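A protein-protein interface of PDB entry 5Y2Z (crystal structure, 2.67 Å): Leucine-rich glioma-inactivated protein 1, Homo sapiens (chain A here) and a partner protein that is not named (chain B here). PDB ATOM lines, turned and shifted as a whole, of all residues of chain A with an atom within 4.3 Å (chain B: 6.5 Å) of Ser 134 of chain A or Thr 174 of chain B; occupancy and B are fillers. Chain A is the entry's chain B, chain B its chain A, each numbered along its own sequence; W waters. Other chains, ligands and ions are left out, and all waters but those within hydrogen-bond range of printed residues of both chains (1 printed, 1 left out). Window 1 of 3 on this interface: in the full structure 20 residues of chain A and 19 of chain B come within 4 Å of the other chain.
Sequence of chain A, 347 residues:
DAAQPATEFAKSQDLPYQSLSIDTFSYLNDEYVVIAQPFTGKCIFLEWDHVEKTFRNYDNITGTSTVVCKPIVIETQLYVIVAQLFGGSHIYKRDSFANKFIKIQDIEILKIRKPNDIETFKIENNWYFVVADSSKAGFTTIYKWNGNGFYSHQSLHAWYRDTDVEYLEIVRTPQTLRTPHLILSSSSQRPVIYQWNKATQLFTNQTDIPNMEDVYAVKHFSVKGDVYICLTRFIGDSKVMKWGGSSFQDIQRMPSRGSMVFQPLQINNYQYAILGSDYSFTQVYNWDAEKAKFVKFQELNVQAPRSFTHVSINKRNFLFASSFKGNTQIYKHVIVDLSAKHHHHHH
O of Asp 173 of chain B sits at hydrogen-bond distance from NZ of Lys 114 of chain A. N of Tyr 176 of chain B is in hydrogen-bond range of OG of Ser 134 of chain A, at 3.0 Å.
The side-chain hydroxyl (OG) of Ser 108 of chain B sits at hydrogen-bond distance from the side-chain hydroxyl (OG1) of Thr 137 of chain B, 3.2 Å away. The side-chain amide nitrogen (NE2) of Gln 140 of chain B lies within hydrogen-bond range of the side-chain hydroxyl (OG) of Ser 108 of chain B. O of Leu 133 of chain B lies within hydrogen-bond range of OG1 of Thr 137 of chain B (3.2 Å). The backbone NH of Ser 134 of chain A lies within hydrogen-bond range of the backbone carbonyl oxygen of Lys 114 of chain A (2.6 Å). The side-chain hydroxyl of Ser 135 of chain A sits at hydrogen-bond distance from the side-chain carboxylate of Asp 133 of chain A (2.6 Å). O of Asp 162 of chain A lies close to N of Ser 134 of chain A, 3.3 Å away.
Among the printed residues, pairs that only touch across the chains: Lys 114 of chain A with Gly 175 of chain B (3.5 Å), Ser 134 of chain A with Thr 174 of chain B (3.9 Å), Ser 134 of chain A with Gly 175 of chain B (3.7 Å), Ser 135 of chain A with Thr 174 of chain B (3.4 Å), Arg 161 of chain A with Ser 108 of chain B (3.8 Å), Arg 161 of chain A with Leu 133 of chain B (3.8 Å) and Arg 161 of chain A with Thr 174 of chain B (3.9 Å).
Of chain A, only Ser 134 (3.9 Å), Ser 135 (3.4 Å) and Arg 161 (3.9 Å) come within 4 Å of Thr 174 of chain B. Printed residues of chain A within 4 Å of Asp 173 of chain B: Lys 114 (3.1 Å). Printed residues of chain B within 4 Å of Lys 114 of chain A: Asp 173 and Gly 175. Of the printed residues of chain A, Leu 133 of chain B touches Arg 161. Printed residues of chain A within 4 Å of Tyr 176 of chain B: Ser 134. Asp 162 of chain A touches none of the printed residues of chain B. The nearest printed residue of chain A that does not touch Leu 133 of chain B is Ser 134 of chain A (7.1 Å).
Printed residues of chain A that touch a printed residue of chain B: Lys 114, Ser 134, Ser 135 and Arg 161. Of the 15 printed residues of chain B, 6 touch a printed residue of chain A. Printed residues of chain B that touch a printed residue of chain A: Ser 108, Leu 133, Asp 173, Thr 174, Gly 175 and Tyr 176. Hydrophobic or aromatic side chains of chain B within 4 Å of the printed part of chain A: Leu 133 and Tyr 176.
Water W1 lies within hydrogen-bond range of NE2 of Gln 140 of chain B (2.8 Å), OG1 of Thr 174 of chain B (2.9 Å), OG of Ser 108 of chain B (2.9 Å), OG1 of Thr 137 of chain B (3.2 Å) and NH2 of Arg 161 of chain A (3.4 Å).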
ATOM      1  N   LYS A 114      21.508 -16.671  -9.366  1.00  0.00           N
ATOM      2  CA  LYS A 114      22.245 -17.257  -8.254  1.00  0.00           C
ATOM      3  C   LYS A 114      23.480 -18.035  -8.717  1.00  0.00           C
ATOM      4  O   LYS A 114      23.502 -19.271  -8.666  1.00  0.00           O
ATOM      5  CB  LYS A 114      21.331 -18.174  -7.441  1.00  0.00           C
ATOM      6  CG  LYS A 114      21.062 -17.695  -6.017  1.00  0.00           C
ATOM      7  CD  LYS A 114      20.006 -16.603  -5.948  1.00  0.00           C
ATOM      8  CE  LYS A 114      19.775 -16.176  -4.505  1.00  0.00           C
ATOM      9  NZ  LYS A 114      18.690 -15.174  -4.366  1.00  0.00           N
ATOM     10  N   ALA A 132      27.659 -21.201 -13.636  1.00  0.00           N
ATOM     11  CA  ALA A 132      26.687 -22.098 -13.040  1.00  0.00           C
ATOM     12  C   ALA A 132      25.707 -21.298 -12.201  1.00  0.00           C
ATOM     13  O   ALA A 132      26.113 -20.557 -11.309  1.00  0.00           O
ATOM     14  CB  ALA A 132      27.377 -23.153 -12.193  1.00  0.00           C
ATOM     15  N   ASP A 133      24.421 -21.430 -12.503  1.00  0.00           N
ATOM     16  CA  ASP A 133      23.383 -20.757 -11.734  1.00  0.00           C
ATOM     17  C   ASP A 133      22.637 -21.788 -10.896  1.00  0.00           C
ATOM     18  O   ASP A 133      22.048 -22.724 -11.433  1.00  0.00           O
ATOM     19  CB  ASP A 133      22.421 -20.005 -12.657  1.00  0.00           C
ATOM     20  CG  ASP A 133      21.626 -18.937 -11.929  1.00  0.00           C
ATOM     21  OD1 ASP A 133      21.180 -19.187 -10.789  1.00  0.00           O
ATOM     22  OD2 ASP A 133      21.461 -17.834 -12.490  1.00  0.00           O
ATOM     23  N   SER A 134      22.669 -21.614  -9.580  1.00  0.00           N
ATOM     24  CA  SER A 134      22.046 -22.570  -8.670  1.00  0.00           C
ATOM     25  C   SER A 134      20.541 -22.327  -8.495  1.00  0.00           C
ATOM     26  O   SER A 134      19.878 -23.039  -7.742  1.00  0.00           O
ATOM     27  CB  SER A 134      22.763 -22.550  -7.316  1.00  0.00           C
ATOM     28  OG  SER A 134      22.846 -21.237  -6.802  1.00  0.00           O
ATOM     29  N   SER A 135      20.008 -21.324  -9.185  1.00  0.00           N
ATOM     30  CA  SER A 135      18.569 -21.047  -9.161  1.00  0.00           C
ATOM     31  C   SER A 135      17.859 -21.744 -10.318  1.00  0.00           C
ATOM     32  O   SER A 135      18.487 -22.099 -11.316  1.00  0.00           O
ATOM     33  CB  SER A 135      18.300 -19.549  -9.230  1.00  0.00           C
ATOM     34  OG  SER A 135      18.581 -19.059 -10.529  1.00  0.00           O
ATOM     35  N   LYS A 136      16.550 -21.933 -10.191  1.00  0.00           N
ATOM     36  CA  LYS A 136      15.782 -22.571 -11.254  1.00  0.00           C
ATOM     37  C   LYS A 136      15.528 -21.649 -12.449  1.00  0.00           C
ATOM     38  O   LYS A 136      15.706 -22.056 -13.599  1.00  0.00           O
ATOM     39  CB  LYS A 136      14.457 -23.079 -10.702  1.00  0.00           C
ATOM     40  CG  LYS A 136      14.442 -24.580 -10.460  1.00  0.00           C
ATOM     41  CD  LYS A 136      13.026 -25.110 -10.328  1.00  0.00           C
ATOM     42  CE  LYS A 136      12.971 -26.606 -10.587  1.00  0.00           C
ATOM     43  NZ  LYS A 136      11.567 -27.108 -10.570  1.00  0.00           N
ATOM     44  N   ARG A 161      19.363 -26.729 -10.729  1.00  0.00           N
ATOM     45  CA  ARG A 161      20.140 -25.989  -9.744  1.00  0.00           C
ATOM     46  C   ARG A 161      21.619 -26.311  -9.874  1.00  0.00           C
ATOM     47  O   ARG A 161      22.197 -26.968  -9.009  1.00  0.00           O
ATOM     48  CB  ARG A 161      19.645 -26.298  -8.329  1.00  0.00           C
ATOM     49  CG  ARG A 161      18.208 -25.847  -8.066  1.00  0.00           C
ATOM     50  CD  ARG A 161      17.820 -26.011  -6.601  1.00  0.00           C
ATOM     51  NE  ARG A 161      16.870 -24.986  -6.175  1.00  0.00           N
ATOM     52  CZ  ARG A 161      15.551 -25.136  -6.184  1.00  0.00           C
ATOM     53  NH1 ARG A 161      15.012 -26.272  -6.600  1.00  0.00           N
ATOM     54  NH2 ARG A 161      14.769 -24.146  -5.776  1.00  0.00           N
ATOM     55  N   ASP A 162      22.231 -25.832 -10.953  1.00  0.00           N
ATOM     56  CA  ASP A 162      23.619 -26.156 -11.238  1.00  0.00           C
ATOM     57  C   ASP A 162      24.557 -25.536 -10.211  1.00  0.00           C
ATOM     58  O   ASP A 162      24.497 -24.341  -9.932  1.00  0.00           O
ATOM     59  CB  ASP A 162      23.993 -25.710 -12.648  1.00  0.00           C
ATOM     60  CG  ASP A 162      23.142 -26.378 -13.708  1.00  0.00           C
ATOM     61  OD1 ASP A 162      23.324 -27.592 -13.945  1.00  0.00           O
ATOM     62  OD2 ASP A 162      22.288 -25.689 -14.302  1.00  0.00           O
ATOM     63  N   SER B 108       9.831 -23.897  -7.441  1.00  0.00           N
ATOM     64  CA  SER B 108      10.053 -25.256  -6.977  1.00  0.00           C
ATOM     65  C   SER B 108       8.754 -25.875  -6.478  1.00  0.00           C
ATOM     66  O   SER B 108       8.717 -27.036  -6.085  1.00  0.00           O
ATOM     67  CB  SER B 108      11.113 -25.275  -5.868  1.00  0.00           C
ATOM     68  OG  SER B 108      10.790 -24.363  -4.837  1.00  0.00           O
ATOM     69  N   LEU B 133      16.600 -27.569   1.658  1.00  0.00           N
ATOM     70  CA  LEU B 133      16.036 -26.881   0.504  1.00  0.00           C
ATOM     71  C   LEU B 133      14.520 -27.061   0.399  1.00  0.00           C
ATOM     72  O   LEU B 133      13.783 -26.092   0.190  1.00  0.00           O
ATOM     73  CB  LEU B 133      16.709 -27.378  -0.778  1.00  0.00           C
ATOM     74  CG  LEU B 133      16.091 -26.911  -2.097  1.00  0.00           C
ATOM     75  CD1 LEU B 133      16.151 -25.396  -2.214  1.00  0.00           C
ATOM     76  CD2 LEU B 133      16.752 -27.585  -3.293  1.00  0.00           C
ATOM     77  N   VAL B 136      12.456 -24.974   2.732  1.00  0.00           N
ATOM     78  CA  VAL B 136      12.232 -23.622   2.232  1.00  0.00           C
ATOM     79  C   VAL B 136      11.102 -23.625   1.203  1.00  0.00           C
ATOM     80  O   VAL B 136      10.268 -22.715   1.174  1.00  0.00           O
ATOM     81  CB  VAL B 136      13.502 -23.030   1.598  1.00  0.00           C
ATOM     82  CG1 VAL B 136      13.205 -21.680   0.962  1.00  0.00           C
ATOM     83  CG2 VAL B 136      14.610 -22.908   2.633  1.00  0.00           C
ATOM     84  N   THR B 137      11.085 -24.654   0.361  1.00  0.00           N
ATOM     85  CA  THR B 137      10.048 -24.813  -0.650  1.00  0.00           C
ATOM     86  C   THR B 137       8.670 -24.916  -0.004  1.00  0.00           C
ATOM     87  O   THR B 137       7.708 -24.292  -0.458  1.00  0.00           O
ATOM     88  CB  THR B 137      10.312 -26.057  -1.520  1.00  0.00           C
ATOM     89  OG1 THR B 137      11.592 -25.931  -2.155  1.00  0.00           O
ATOM     90  CG2 THR B 137       9.238 -26.213  -2.583  1.00  0.00           C
ATOM     91  N   GLN B 140       7.573 -21.416   1.532  1.00  0.00           N
ATOM     92  CA  GLN B 140       7.048 -20.455   0.565  1.00  0.00           C
ATOM     93  C   GLN B 140       5.733 -20.935  -0.054  1.00  0.00           C
ATOM     94  O   GLN B 140       4.920 -20.131  -0.503  1.00  0.00           O
ATOM     95  CB  GLN B 140       8.095 -20.170  -0.518  1.00  0.00           C
ATOM     96  CG  GLN B 140       8.594 -21.393  -1.249  1.00  0.00           C
ATOM     97  CD  GLN B 140       9.839 -21.110  -2.074  1.00  0.00           C
ATOM     98  OE1 GLN B 140      10.402 -20.022  -2.011  1.00  0.00           O
ATOM     99  NE2 GLN B 140      10.281 -22.103  -2.837  1.00  0.00           N
ATOM    100  N   CYS B 169      15.786 -13.786   1.026  1.00  0.00           N
ATOM    101  CA  CYS B 169      14.580 -14.126   1.777  1.00  0.00           C
ATOM    102  C   CYS B 169      13.761 -15.244   1.123  1.00  0.00           C
ATOM    103  O   CYS B 169      13.932 -15.561  -0.055  1.00  0.00           O
ATOM    104  CB  CYS B 169      13.707 -12.883   1.958  1.00  0.00           C
ATOM    105  SG  CYS B 169      14.455 -11.585   2.977  1.00  0.00           S
ATOM    106  N   ILE B 170      12.871 -15.837   1.912  1.00  0.00           N
ATOM    107  CA  ILE B 170      12.128 -17.028   1.512  1.00  0.00           C
ATOM    108  C   ILE B 170      11.287 -16.862   0.251  1.00  0.00           C
ATOM    109  O   ILE B 170      11.288 -17.733  -0.616  1.00  0.00           O
ATOM    110  CB  ILE B 170      11.219 -17.498   2.654  1.00  0.00           C
ATOM    111  CG1 ILE B 170      12.072 -17.829   3.874  1.00  0.00           C
ATOM    112  CG2 ILE B 170      10.418 -18.723   2.248  1.00  0.00           C
ATOM    113  CD1 ILE B 170      11.276 -18.308   5.027  1.00  0.00           C
ATOM    114  N   GLY B 172      11.770 -15.080  -2.180  1.00  0.00           N
ATOM    115  CA  GLY B 172      12.593 -14.765  -3.335  1.00  0.00           C
ATOM    116  C   GLY B 172      13.081 -16.018  -4.040  1.00  0.00           C
ATOM    117  O   GLY B 172      12.870 -17.132  -3.554  1.00  0.00           O
ATOM    118  N   ASP B 173      13.735 -15.837  -5.186  1.00  0.00           N
ATOM    119  CA  ASP B 173      14.284 -16.963  -5.936  1.00  0.00           C
ATOM    120  C   ASP B 173      15.338 -17.686  -5.108  1.00  0.00           C
ATOM    121  O   ASP B 173      16.257 -17.065  -4.576  1.00  0.00           O
ATOM    122  CB  ASP B 173      14.887 -16.500  -7.263  1.00  0.00           C
ATOM    123  CG  ASP B 173      13.881 -15.800  -8.151  1.00  0.00           C
ATOM    124  OD1 ASP B 173      12.680 -16.138  -8.076  1.00  0.00           O
ATOM    125  OD2 ASP B 173      14.296 -14.919  -8.934  1.00  0.00           O
ATOM    126  N   THR B 174      15.205 -19.003  -5.012  1.00  0.00           N
ATOM    127  CA  THR B 174      16.093 -19.795  -4.175  1.00  0.00           C
ATOM    128  C   THR B 174      17.311 -20.293  -4.943  1.00  0.00           C
ATOM    129  O   THR B 174      17.191 -20.767  -6.073  1.00  0.00           O
ATOM    130  CB  THR B 174      15.360 -21.007  -3.579  1.00  0.00           C
ATOM    131  OG1 THR B 174      14.070 -20.606  -3.103  1.00  0.00           O
ATOM    132  CG2 THR B 174      16.159 -21.593  -2.436  1.00  0.00           C
ATOM    133  N   GLY B 175      18.478 -20.199  -4.312  1.00  0.00           N
ATOM    134  CA  GLY B 175      19.709 -20.709  -4.886  1.00  0.00           C
ATOM    135  C   GLY B 175      20.391 -21.667  -3.929  1.00  0.00           C
ATOM    136  O   GLY B 175      19.751 -22.207  -3.031  1.00  0.00           O
ATOM    137  N   TYR B 176      21.688 -21.875  -4.106  1.00  0.00           N
ATOM    138  CA  TYR B 176      22.421 -22.791  -3.243  1.00  0.00           C
ATOM    139  C   TYR B 176      22.404 -22.327  -1.798  1.00  0.00           C
ATOM    140  O   TYR B 176      22.077 -23.100  -0.897  1.00  0.00           O
ATOM    141  CB  TYR B 176      23.861 -22.960  -3.714  1.00  0.00           C
ATOM    142  CG  TYR B 176      24.659 -23.874  -2.813  1.00  0.00           C
ATOM    143  CD1 TYR B 176      24.384 -25.239  -2.761  1.00  0.00           C
ATOM    144  CD2 TYR B 176      25.687 -23.380  -2.016  1.00  0.00           C
ATOM    145  CE1 TYR B 176      25.106 -26.086  -1.942  1.00  0.00           C
ATOM    146  CE2 TYR B 176      26.416 -24.222  -1.191  1.00  0.00           C
ATOM    147  CZ  TYR B 176      26.118 -25.574  -1.159  1.00  0.00           C
ATOM    148  OH  TYR B 176      26.833 -26.423  -0.346  1.00  0.00           O
ATOM    149  N   TYR B 177      22.772 -21.069  -1.577  1.00  0.00           N
ATOM    150  CA  TYR B 177      22.719 -20.499  -0.239  1.00  0.00           C
ATOM    151  C   TYR B 177      21.277 -20.148   0.140  1.00  0.00           C
ATOM    152  O   TYR B 177      20.726 -19.146  -0.320  1.00  0.00           O
ATOM    153  CB  TYR B 177      23.627 -19.278  -0.148  1.00  0.00           C
ATOM    154  CG  TYR B 177      25.081 -19.599  -0.410  1.00  0.00           C
ATOM    155  CD1 TYR B 177      25.870 -20.181   0.571  1.00  0.00           C
ATOM    156  CD2 TYR B 177      25.667 -19.314  -1.635  1.00  0.00           C
ATOM    157  CE1 TYR B 177      27.197 -20.478   0.337  1.00  0.00           C
ATOM    158  CE2 TYR B 177      26.999 -19.603  -1.877  1.00  0.00           C
ATOM    159  CZ  TYR B 177      27.759 -20.185  -0.888  1.00  0.00           C
ATOM    160  OH  TYR B 177      29.086 -20.482  -1.123  1.00  0.00           O
ATOM    161  N   LEU B 178      20.688 -20.974   0.999  1.00  0.00           N
ATOM    162  CA  LEU B 178      19.262 -20.902   1.310  1.00  0.00           C
ATOM    163  C   LEU B 178      18.893 -19.752   2.231  1.00  0.00           C
ATOM    164  O   LEU B 178      19.639 -19.417   3.148  1.00  0.00           O
ATOM    165  CB  LEU B 178      18.800 -22.215   1.945  1.00  0.00           C
ATOM    166  CG  LEU B 178      19.080 -23.485   1.143  1.00  0.00           C
ATOM    167  CD1 LEU B 178      18.591 -24.702   1.899  1.00  0.00           C
ATOM    168  CD2 LEU B 178      18.427 -23.397  -0.224  1.00  0.00           C
ATOM    169  N   PRO B 179      17.719 -19.148   1.993  1.00  0.00           N
ATOM    170  CA  PRO B 179      17.195 -18.084   2.852  1.00  0.00           C
ATOM    171  C   PRO B 179      16.702 -18.642   4.180  1.00  0.00           C
ATOM    172  O   PRO B 179      16.452 -19.843   4.290  1.00  0.00           O
ATOM    173  CB  PRO B 179      16.037 -17.517   2.036  1.00  0.00           C
ATOM    174  CG  PRO B 179      15.563 -18.677   1.233  1.00  0.00           C
ATOM    175  CD  PRO B 179      16.783 -19.487   0.906  1.00  0.00           C
HETATM  176  O   HOH W   1      12.799 -23.158  -3.171  1.00  0.00           O
